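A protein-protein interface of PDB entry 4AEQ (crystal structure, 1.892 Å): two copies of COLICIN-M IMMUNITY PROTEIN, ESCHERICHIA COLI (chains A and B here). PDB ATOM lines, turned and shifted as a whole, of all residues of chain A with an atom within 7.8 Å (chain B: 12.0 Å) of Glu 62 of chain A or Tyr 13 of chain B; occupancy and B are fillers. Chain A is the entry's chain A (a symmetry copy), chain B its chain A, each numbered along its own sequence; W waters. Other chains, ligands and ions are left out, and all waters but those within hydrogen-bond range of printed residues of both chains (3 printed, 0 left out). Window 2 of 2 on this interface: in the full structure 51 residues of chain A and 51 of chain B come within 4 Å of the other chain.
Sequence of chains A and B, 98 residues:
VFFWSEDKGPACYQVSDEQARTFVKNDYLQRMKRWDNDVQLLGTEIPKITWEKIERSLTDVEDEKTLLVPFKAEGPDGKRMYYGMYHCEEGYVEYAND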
ATOM      1  N   ARG A  56      30.555 -13.030  -4.269  1.00  0.00           N
ATOM      2  CA  ARG A  56      29.743 -13.836  -5.162  1.00  0.00           C
ATOM      3  C   ARG A  56      29.312 -15.096  -4.437  1.00  0.00           C
ATOM      4  O   ARG A  56      30.013 -15.574  -3.543  1.00  0.00           O
ATOM      5  CB  ARG A  56      30.509 -14.166  -6.444  1.00  0.00           C
ATOM      6  CG  ARG A  56      31.893 -14.740  -6.215  1.00  0.00           C
ATOM      7  CD  ARG A  56      32.735 -14.646  -7.480  1.00  0.00           C
ATOM      8  NE  ARG A  56      32.120 -15.353  -8.598  1.00  0.00           N
ATOM      9  CZ  ARG A  56      32.610 -15.364  -9.835  1.00  0.00           C
ATOM     10  NH1 ARG A  56      33.727 -14.705 -10.119  1.00  0.00           N
ATOM     11  NH2 ARG A  56      31.987 -16.037 -10.791  1.00  0.00           N
ATOM     12  N   SER A  57      28.156 -15.626  -4.814  1.00  0.00           N
ATOM     13  CA  SER A  57      27.610 -16.795  -4.144  1.00  0.00           C
ATOM     14  C   SER A  57      28.543 -17.986  -4.313  1.00  0.00           C
ATOM     15  O   SER A  57      29.050 -18.237  -5.405  1.00  0.00           O
ATOM     16  CB  SER A  57      26.217 -17.127  -4.683  1.00  0.00           C
ATOM     17  OG  SER A  57      25.581 -18.109  -3.885  1.00  0.00           O
ATOM     18  N   THR A  59      27.467 -20.978  -3.579  1.00  0.00           N
ATOM     19  CA  THR A  59      26.565 -22.086  -3.877  1.00  0.00           C
ATOM     20  C   THR A  59      25.603 -21.732  -5.004  1.00  0.00           C
ATOM     21  O   THR A  59      25.268 -20.564  -5.200  1.00  0.00           O
ATOM     22  CB  THR A  59      25.741 -22.498  -2.640  1.00  0.00           C
ATOM     23  OG1 THR A  59      25.055 -21.353  -2.116  1.00  0.00           O
ATOM     24  CG2 THR A  59      26.642 -23.085  -1.568  1.00  0.00           C
ATOM     25  N   ASP A  60      25.159 -22.752  -5.734  1.00  0.00           N
ATOM     26  CA  ASP A  60      24.209 -22.563  -6.826  1.00  0.00           C
ATOM     27  C   ASP A  60      24.720 -21.501  -7.789  1.00  0.00           C
ATOM     28  O   ASP A  60      23.963 -20.650  -8.257  1.00  0.00           O
ATOM     29  CB  ASP A  60      22.845 -22.158  -6.268  1.00  0.00           C
ATOM     30  CG  ASP A  60      22.405 -23.037  -5.112  1.00  0.00           C
ATOM     31  OD1 ASP A  60      22.604 -24.269  -5.187  1.00  0.00           O
ATOM     32  OD2 ASP A  60      21.870 -22.494  -4.121  1.00  0.00           O
ATOM     33  N   VAL A  61      26.014 -21.566  -8.088  1.00  0.00           N
ATOM     34  CA  VAL A  61      26.691 -20.519  -8.844  1.00  0.00           C
ATOM     35  C   VAL A  61      26.167 -20.356 -10.269  1.00  0.00           C
ATOM     36  O   VAL A  61      26.303 -19.291 -10.862  1.00  0.00           O
ATOM     37  CB  VAL A  61      28.208 -20.760  -8.896  1.00  0.00           C
ATOM     38  CG1 VAL A  61      28.796 -20.730  -7.494  1.00  0.00           C
ATOM     39  CG2 VAL A  61      28.510 -22.086  -9.578  1.00  0.00           C
ATOM     40  N   GLU A  62      25.565 -21.407 -10.814  1.00  0.00           N
ATOM     41  CA  GLU A  62      25.039 -21.347 -12.174  1.00  0.00           C
ATOM     42  C   GLU A  62      23.812 -20.441 -12.251  1.00  0.00           C
ATOM     43  O   GLU A  62      23.329 -20.120 -13.338  1.00  0.00           O
ATOM     44  CB  GLU A  62      24.731 -22.751 -12.700  1.00  0.00           C
ATOM     45  CG  GLU A  62      25.985 -23.578 -12.959  1.00  0.00           C
ATOM     46  CD  GLU A  62      25.703 -25.065 -13.111  1.00  0.00           C
ATOM     47  OE1 GLU A  62      24.552 -25.489 -12.870  1.00  0.00           O
ATOM     48  OE2 GLU A  62      26.640 -25.811 -13.468  1.00  0.00           O
ATOM     49  N   ASP A  63      23.320 -20.025 -11.086  1.00  0.00           N
ATOM     50  CA  ASP A  63      22.175 -19.124 -11.011  1.00  0.00           C
ATOM     51  C   ASP A  63      22.567 -17.645 -11.078  1.00  0.00           C
ATOM     52  O   ASP A  63      21.695 -16.781 -11.154  1.00  0.00           O
ATOM     53  CB  ASP A  63      21.371 -19.378  -9.731  1.00  0.00           C
ATOM     54  CG  ASP A  63      20.870 -20.807  -9.626  1.00  0.00           C
ATOM     55  OD1 ASP A  63      20.745 -21.479 -10.674  1.00  0.00           O
ATOM     56  OD2 ASP A  63      20.599 -21.257  -8.492  1.00  0.00           O
ATOM     57  N   GLU A  64      23.868 -17.352 -11.062  1.00  0.00           N
ATOM     58  CA  GLU A  64      24.326 -15.964 -11.071  1.00  0.00           C
ATOM     59  C   GLU A  64      24.167 -15.386 -12.462  1.00  0.00           C
ATOM     60  O   GLU A  64      24.758 -15.893 -13.412  1.00  0.00           O
ATOM     61  CB  GLU A  64      25.820 -15.888 -10.753  1.00  0.00           C
ATOM     62  CG  GLU A  64      26.245 -16.227  -9.342  1.00  0.00           C
ATOM     63  CD  GLU A  64      27.760 -16.242  -9.212  1.00  0.00           C
ATOM     64  OE1 GLU A  64      28.432 -16.708 -10.159  1.00  0.00           O
ATOM     65  OE2 GLU A  64      28.280 -15.772  -8.178  1.00  0.00           O
ATOM     66  N   LYS A  65      23.370 -14.332 -12.593  1.00  0.00           N
ATOM     67  CA  LYS A  65      23.333 -13.582 -13.843  1.00  0.00           C
ATOM     68  C   LYS A  65      24.235 -12.345 -13.852  1.00  0.00           C
ATOM     69  O   LYS A  65      24.484 -11.751 -14.903  1.00  0.00           O
ATOM     70  CB  LYS A  65      21.891 -13.207 -14.184  1.00  0.00           C
ATOM     71  CG  LYS A  65      20.985 -14.415 -14.402  1.00  0.00           C
ATOM     72  CD  LYS A  65      21.463 -15.249 -15.583  1.00  0.00           C
ATOM     73  CE  LYS A  65      20.573 -16.463 -15.827  1.00  0.00           C
ATOM     74  NZ  LYS A  65      21.017 -17.659 -15.054  1.00  0.00           N
ATOM     75  N   THR A  66      24.748 -11.975 -12.683  1.00  0.00           N
ATOM     76  CA  THR A  66      25.486 -10.725 -12.547  1.00  0.00           C
ATOM     77  C   THR A  66      26.594 -10.835 -11.509  1.00  0.00           C
ATOM     78  O   THR A  66      26.420 -11.466 -10.465  1.00  0.00           O
ATOM     79  CB  THR A  66      24.547  -9.564 -12.145  1.00  0.00           C
ATOM     80  OG1 THR A  66      23.580  -9.344 -13.180  1.00  0.00           O
ATOM     81  CG2 THR A  66      25.337  -8.286 -11.923  1.00  0.00           C
ATOM     82  N   LEU A  67      27.732 -10.218 -11.804  1.00  0.00           N
ATOM     83  CA  LEU A  67      28.807 -10.112 -10.831  1.00  0.00           C
ATOM     84  C   LEU A  67      28.926  -8.667 -10.390  1.00  0.00           C
ATOM     85  O   LEU A  67      29.024  -7.768 -11.220  1.00  0.00           O
ATOM     86  CB  LEU A  67      30.137 -10.566 -11.430  1.00  0.00           C
ATOM     87  CG  LEU A  67      30.302 -12.055 -11.731  1.00  0.00           C
ATOM     88  CD1 LEU A  67      31.720 -12.329 -12.225  1.00  0.00           C
ATOM     89  CD2 LEU A  67      29.989 -12.881 -10.492  1.00  0.00           C
ATOM     90  N   CYS A  88      27.296 -10.867 -17.288  1.00  0.00           N
ATOM     91  CA  CYS A  88      28.364 -11.573 -17.981  1.00  0.00           C
ATOM     92  C   CYS A  88      27.949 -12.016 -19.379  1.00  0.00           C
ATOM     93  O   CYS A  88      28.658 -11.771 -20.355  1.00  0.00           O
ATOM     94  CB  CYS A  88      28.823 -12.769 -17.142  1.00  0.00           C
ATOM     95  SG  CYS A  88      29.107 -12.368 -15.382  1.00  0.00           S
ATOM     96  N   GLU A  89      26.793 -12.660 -19.470  1.00  0.00           N
ATOM     97  CA  GLU A  89      26.303 -13.182 -20.740  1.00  0.00           C
ATOM     98  C   GLU A  89      25.974 -12.076 -21.736  1.00  0.00           C
ATOM     99  O   GLU A  89      26.210 -12.225 -22.935  1.00  0.00           O
ATOM    100  CB  GLU A  89      25.084 -14.081 -20.517  1.00  0.00           C
ATOM    101  CG  GLU A  89      25.431 -15.446 -19.942  1.00  0.00           C
ATOM    102  CD  GLU A  89      24.235 -16.150 -19.328  1.00  0.00           C
ATOM    103  OE1 GLU A  89      23.221 -15.475 -19.051  1.00  0.00           O
ATOM    104  OE2 GLU A  89      24.313 -17.380 -19.121  1.00  0.00           O
ATOM    105  N   LYS B   8      26.301 -15.187 -27.205  1.00  0.00           N
ATOM    106  CA  LYS B   8      26.316 -14.476 -25.931  1.00  0.00           C
ATOM    107  C   LYS B   8      27.643 -14.662 -25.201  1.00  0.00           C
ATOM    108  O   LYS B   8      28.403 -15.579 -25.506  1.00  0.00           O
ATOM    109  CB  LYS B   8      25.161 -14.940 -25.037  1.00  0.00           C
ATOM    110  CG  LYS B   8      25.274 -16.373 -24.535  1.00  0.00           C
ATOM    111  CD  LYS B   8      24.799 -17.373 -25.579  1.00  0.00           C
ATOM    112  CE  LYS B   8      24.976 -18.803 -25.089  1.00  0.00           C
ATOM    113  NZ  LYS B   8      24.431 -19.800 -26.050  1.00  0.00           N
ATOM    114  N   GLY B   9      27.914 -13.794 -24.230  1.00  0.00           N
ATOM    115  CA  GLY B   9      29.140 -13.876 -23.460  1.00  0.00           C
ATOM    116  C   GLY B   9      29.146 -15.057 -22.511  1.00  0.00           C
ATOM    117  O   GLY B   9      28.227 -15.873 -22.518  1.00  0.00           O
ATOM    118  N   PRO B  10      30.194 -15.159 -21.685  1.00  0.00           N
ATOM    119  CA  PRO B  10      30.323 -16.270 -20.742  1.00  0.00           C
ATOM    120  C   PRO B  10      29.290 -16.181 -19.628  1.00  0.00           C
ATOM    121  O   PRO B  10      28.846 -15.086 -19.286  1.00  0.00           O
ATOM    122  CB  PRO B  10      31.721 -16.060 -20.160  1.00  0.00           C
ATOM    123  CG  PRO B  10      31.946 -14.594 -20.258  1.00  0.00           C
ATOM    124  CD  PRO B  10      31.286 -14.180 -21.541  1.00  0.00           C
ATOM    125  N   ALA B  11      28.911 -17.325 -19.071  1.00  0.00           N
ATOM    126  CA  ALA B  11      28.094 -17.332 -17.868  1.00  0.00           C
ATOM    127  C   ALA B  11      28.959 -16.841 -16.710  1.00  0.00           C
ATOM    128  O   ALA B  11      30.172 -17.043 -16.708  1.00  0.00           O
ATOM    129  CB  ALA B  11      27.563 -18.729 -17.591  1.00  0.00           C
ATOM    130  N   CYS B  12      28.345 -16.185 -15.731  1.00  0.00           N
ATOM    131  CA  CYS B  12      29.109 -15.609 -14.628  1.00  0.00           C
ATOM    132  C   CYS B  12      29.979 -16.628 -13.893  1.00  0.00           C
ATOM    133  O   CYS B  12      31.081 -16.302 -13.451  1.00  0.00           O
ATOM    134  CB  CYS B  12      28.186 -14.868 -13.661  1.00  0.00           C
ATOM    135  SG  CYS B  12      27.597 -13.312 -14.342  1.00  0.00           S
ATOM    136  N   TYR B  13      29.495 -17.861 -13.770  1.00  0.00           N
ATOM    137  CA  TYR B  13      30.252 -18.884 -13.053  1.00  0.00           C
ATOM    138  C   TYR B  13      31.508 -19.301 -13.818  1.00  0.00           C
ATOM    139  O   TYR B  13      32.392 -19.954 -13.269  1.00  0.00           O
ATOM    140  CB  TYR B  13      29.381 -20.102 -12.719  1.00  0.00           C
ATOM    141  CG  TYR B  13      28.995 -20.966 -13.901  1.00  0.00           C
ATOM    142  CD1 TYR B  13      29.812 -22.008 -14.324  1.00  0.00           C
ATOM    143  CD2 TYR B  13      27.796 -20.758 -14.575  1.00  0.00           C
ATOM    144  CE1 TYR B  13      29.454 -22.808 -15.397  1.00  0.00           C
ATOM    145  CE2 TYR B  13      27.432 -21.553 -15.649  1.00  0.00           C
ATOM    146  CZ  TYR B  13      28.264 -22.576 -16.054  1.00  0.00           C
ATOM    147  OH  TYR B  13      27.903 -23.366 -17.120  1.00  0.00           O
ATOM    148  N   GLN B  14      31.581 -18.911 -15.085  1.00  0.00           N
ATOM    149  CA  GLN B  14      32.762 -19.163 -15.896  1.00  0.00           C
ATOM    150  C   GLN B  14      33.711 -17.966 -15.887  1.00  0.00           C
ATOM    151  O   GLN B  14      34.792 -18.015 -16.476  1.00  0.00           O
ATOM    152  CB  GLN B  14      32.350 -19.506 -17.328  1.00  0.00           C
ATOM    153  CG  GLN B  14      31.435 -20.715 -17.414  1.00  0.00           C
ATOM    154  CD  GLN B  14      30.877 -20.927 -18.806  1.00  0.00           C
ATOM    155  OE1 GLN B  14      30.587 -19.971 -19.523  1.00  0.00           O
ATOM    156  NE2 GLN B  14      30.726 -22.187 -19.195  1.00  0.00           N
ATOM    157  N   VAL B  15      33.306 -16.896 -15.210  1.00  0.00           N
ATOM    158  CA  VAL B  15      34.105 -15.676 -15.157  1.00  0.00           C
ATOM    159  C   VAL B  15      34.811 -15.540 -13.816  1.00  0.00           C
ATOM    160  O   VAL B  15      34.165 -15.432 -12.778  1.00  0.00           O
ATOM    161  CB  VAL B  15      33.235 -14.424 -15.389  1.00  0.00           C
ATOM    162  CG1 VAL B  15      34.063 -13.155 -15.221  1.00  0.00           C
ATOM    163  CG2 VAL B  15      32.603 -14.472 -16.769  1.00  0.00           C
ATOM    164  N   SER B  16      36.140 -15.553 -13.838  1.00  0.00           N
ATOM    165  CA  SER B  16      36.925 -15.380 -12.622  1.00  0.00           C
ATOM    166  C   SER B  16      36.895 -13.929 -12.155  1.00  0.00           C
ATOM    167  O   SER B  16      36.580 -13.027 -12.933  1.00  0.00           O
ATOM    168  CB  SER B  16      38.372 -15.822 -12.846  1.00  0.00           C
ATOM    169  OG  SER B  16      39.051 -14.906 -13.688  1.00  0.00           O
ATOM    170  N   ASP B  17      37.211 -13.709 -10.883  1.00  0.00           N
ATOM    171  CA  ASP B  17      37.287 -12.354 -10.339  1.00  0.00           C
ATOM    172  C   ASP B  17      38.209 -11.476 -11.183  1.00  0.00           C
ATOM    173  O   ASP B  17      37.922 -10.303 -11.408  1.00  0.00           O
ATOM    174  CB  ASP B  17      37.780 -12.380  -8.888  1.00  0.00           C
ATOM    175  CG  ASP B  17      36.685 -12.752  -7.903  1.00  0.00           C
ATOM    176  OD1 ASP B  17      35.570 -13.109  -8.346  1.00  0.00           O
ATOM    177  OD2 ASP B  17      36.944 -12.690  -6.682  1.00  0.00           O
ATOM    178  N   GLU B  18      39.317 -12.051 -11.643  1.00  0.00           N
ATOM    179  CA  GLU B  18      40.300 -11.311 -12.430  1.00  0.00           C
ATOM    180  C   GLU B  18      39.751 -10.903 -13.799  1.00  0.00           C
ATOM    181  O   GLU B  18      39.959  -9.771 -14.249  1.00  0.00           O
ATOM    182  CB  GLU B  18      41.580 -12.136 -12.584  1.00  0.00           C
ATOM    183  CG  GLU B  18      42.787 -11.343 -13.055  1.00  0.00           C
ATOM    184  CD  GLU B  18      42.900 -11.293 -14.565  1.00  0.00           C
ATOM    185  OE1 GLU B  18      42.110 -11.982 -15.244  1.00  0.00           O
ATOM    186  OE2 GLU B  18      43.784 -10.572 -15.072  1.00  0.00           O
ATOM    187  N   GLN B  19      39.058 -11.831 -14.457  1.00  0.00           N
ATOM    188  CA  GLN B  19      38.405 -11.548 -15.736  1.00  0.00           C
ATOM    189  C   GLN B  19      37.346 -10.469 -15.582  1.00  0.00           C
ATOM    190  O   GLN B  19      37.252  -9.558 -16.405  1.00  0.00           O
ATOM    191  CB  GLN B  19      37.746 -12.807 -16.300  1.00  0.00           C
ATOM    192  CG  GLN B  19      38.713 -13.827 -16.865  1.00  0.00           C
ATOM    193  CD  GLN B  19      38.022 -15.110 -17.283  1.00  0.00           C
ATOM    194  OE1 GLN B  19      37.355 -15.758 -16.477  1.00  0.00           O
ATOM    195  NE2 GLN B  19      38.176 -15.482 -18.548  1.00  0.00           N
ATOM    196  N   ALA B  20      36.541 -10.587 -14.531  1.00  0.00           N
ATOM    197  CA  ALA B  20      35.492  -9.615 -14.252  1.00  0.00           C
ATOM    198  C   ALA B  20      36.087  -8.230 -14.016  1.00  0.00           C
ATOM    199  O   ALA B  20      35.598  -7.239 -14.553  1.00  0.00           O
ATOM    200  CB  ALA B  20      34.670 -10.052 -13.047  1.00  0.00           C
HETATM  201  O   HOH W   1      25.494 -15.892 -16.069  1.00  0.00           O
HETATM  202  O   HOH W   2      24.933 -13.374 -17.026  1.00  0.00           O
HETATM  203  O   HOH W   3      26.441 -18.161 -13.595  1.00  0.00           O
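Water W2 lies within hydrogen-bond range of the backbone carbonyl oxygen of Lys 65 of chain A, the backbone NH of Glu 89 of chain A, the backbone NH of Cys 88 of chain A and the side-chain sulfur of Cys 12 of chain B.
Water W1 bridges the backbone carbonyl oxygen (O) of Glu 64 of chain A (2.8 Å) and the backbone NH (N) of Cys 12 of chain B (2.9 Å).
Water W3 lies within hydrogen-bond range of O of Glu 64 of chain A (2.8 Å), O of Val 61 of chain A (3.0 Å), N of Tyr 13 of chain B (3.1 Å) and N of Cys 12 of chain B (3.5 Å).
Of chain B, only Tyr 13 (3.7 Å) comes within 4 Å of Glu 62 of chain A.
Tyr 13 of chain B touches just these residues of chain A: Val 61, Glu 62 and Glu 64.
Printed residues of chain B within 4 Å of Val 61 of chain A: Tyr 13.
No residue of chain B comes within 4 Å of Asp 63 of chain A.
Glu 64 of chain A touches just these residues of chain B: Cys 12 (3.6 Å) and Tyr 13 (3.9 Å).
Of the printed residues of chain A, Pro 10 of chain B touches Cys 88 and Glu 89.
Of the printed residues of chain A, Ala 11 of chain B touches Glu 89 (3.8 Å).
Glu 18 of chain B touches none of the printed residues of chain A.
The nearest residue of chain A that does not touch Tyr 13 of chain B is Arg 56 of chain A (4.03 Å).
The nearest printed residue of chain B that does not touch Lys 65 of chain A is Ala 11 of chain B (7.0 Å).
Arg 56 of chain A touches Ser 16 of chain B (NH1 to C, 3.8 Å).
Val 61 of chain A touches Tyr 13 of chain B (O to CB, 3.7 Å).
CG of Glu 62 of chain A touches CE2 of Tyr 13 of chain B (3.7 Å).
Tyr 13 of chain B touches Glu 64 of chain A (N to OE1, 3.9 Å).
CG of Leu 67 of chain A touches SG of Cys 12 of chain B (3.96 Å).
CD1 of Leu 67 of chain A touches CG1 of Val 15 of chain B, at 3.9 Å.
CB of Ala 20 of chain B touches CD1 of Leu 67 of chain A, at 3.8 Å.
Cys 88 of chain A touches Gly 9 of chain B (O to CA, 3.8 Å).
Lys 8 of chain B touches Glu 89 of chain A.
Glu 89 of chain A touches Ala 11 of chain B (OE2 to CB, 3.8 Å).
No position is printed for both chains.
Of the 20 pairs that touch across the chains among the printed residues, none has its exchanged pair printed and touching as well.
O of Cys 88 of chain A lies close to O of Pro 10 of chain B, 3.5 Å away.
The backbone carbonyl oxygen (O) of Pro 10 of chain B sits at hydrogen-bond distance from the backbone NH (N) of Glu 89 of chain A (3.2 Å).
The backbone carbonyl oxygen of Cys 12 of chain B lies within hydrogen-bond range of the guanidinium group of Arg 56 of chain A, at 2.8 Å.
N of Gly 9 of chain B sits at hydrogen-bond distance from O of Glu 89 of chain A, at 2.7 Å.
NH1 of Arg 56 of chain A is in salt-bridge range of OD1 of Asp 17 of chain B (3.0 Å).
SG of Cys 12 of chain B is in hydrogen-bond range of N of Thr 66 of chain A, at 3.6 Å.
O of Lys 65 of chain A lies close to SG of Cys 12 of chain B (3.5 Å).
The backbone carbonyl oxygen of Val 15 of chain B lies within hydrogen-bond range of the guanidinium group of Arg 56 of chain A (2.8 Å).
SG of Cys 12 of chain B forms a disulfide with SG of Cys 88 of chain A (2.1 Å).
The side-chain amide oxygen (OE1) of Gln 14 of chain B is in hydrogen-bond range of the backbone NH (N) of Ala 11 of chain B (3.2 Å).
The side-chain amide oxygen (OE1) of Gln 19 of chain B sits at hydrogen-bond distance from the backbone NH (N) of Ser 16 of chain B (2.9 Å).
The side-chain carboxylate (OE1) of Glu 64 of chain A lies within salt-bridge range of the guanidinium group (NH2) of Arg 56 of chain A (3.7 Å).
The side-chain carboxylate of Glu 64 of chain A lies within hydrogen-bond range of the backbone NH of Ser 57 of chain A (3.4 Å).
Printed residues of chain B that touch a printed residue of chain A: Lys 8, Gly 9, Pro 10, Ala 11, Cys 12, Tyr 13, Val 15, Ser 16, Asp 17 and Ala 20.
Hydrophobic or aromatic side chains of chain B within 4 Å of the printed part of chain A: Pro 10, Ala 11, Tyr 13, Val 15 and Ala 20.
Of the 13 printed residues of chain A, 9 touch a printed residue of chain B.
Hydrophobic or aromatic side chains of chain A that line the printed part of chain B: Val 61 and Leu 67.
Among the printed residues, 20 pairs touch across the chains.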
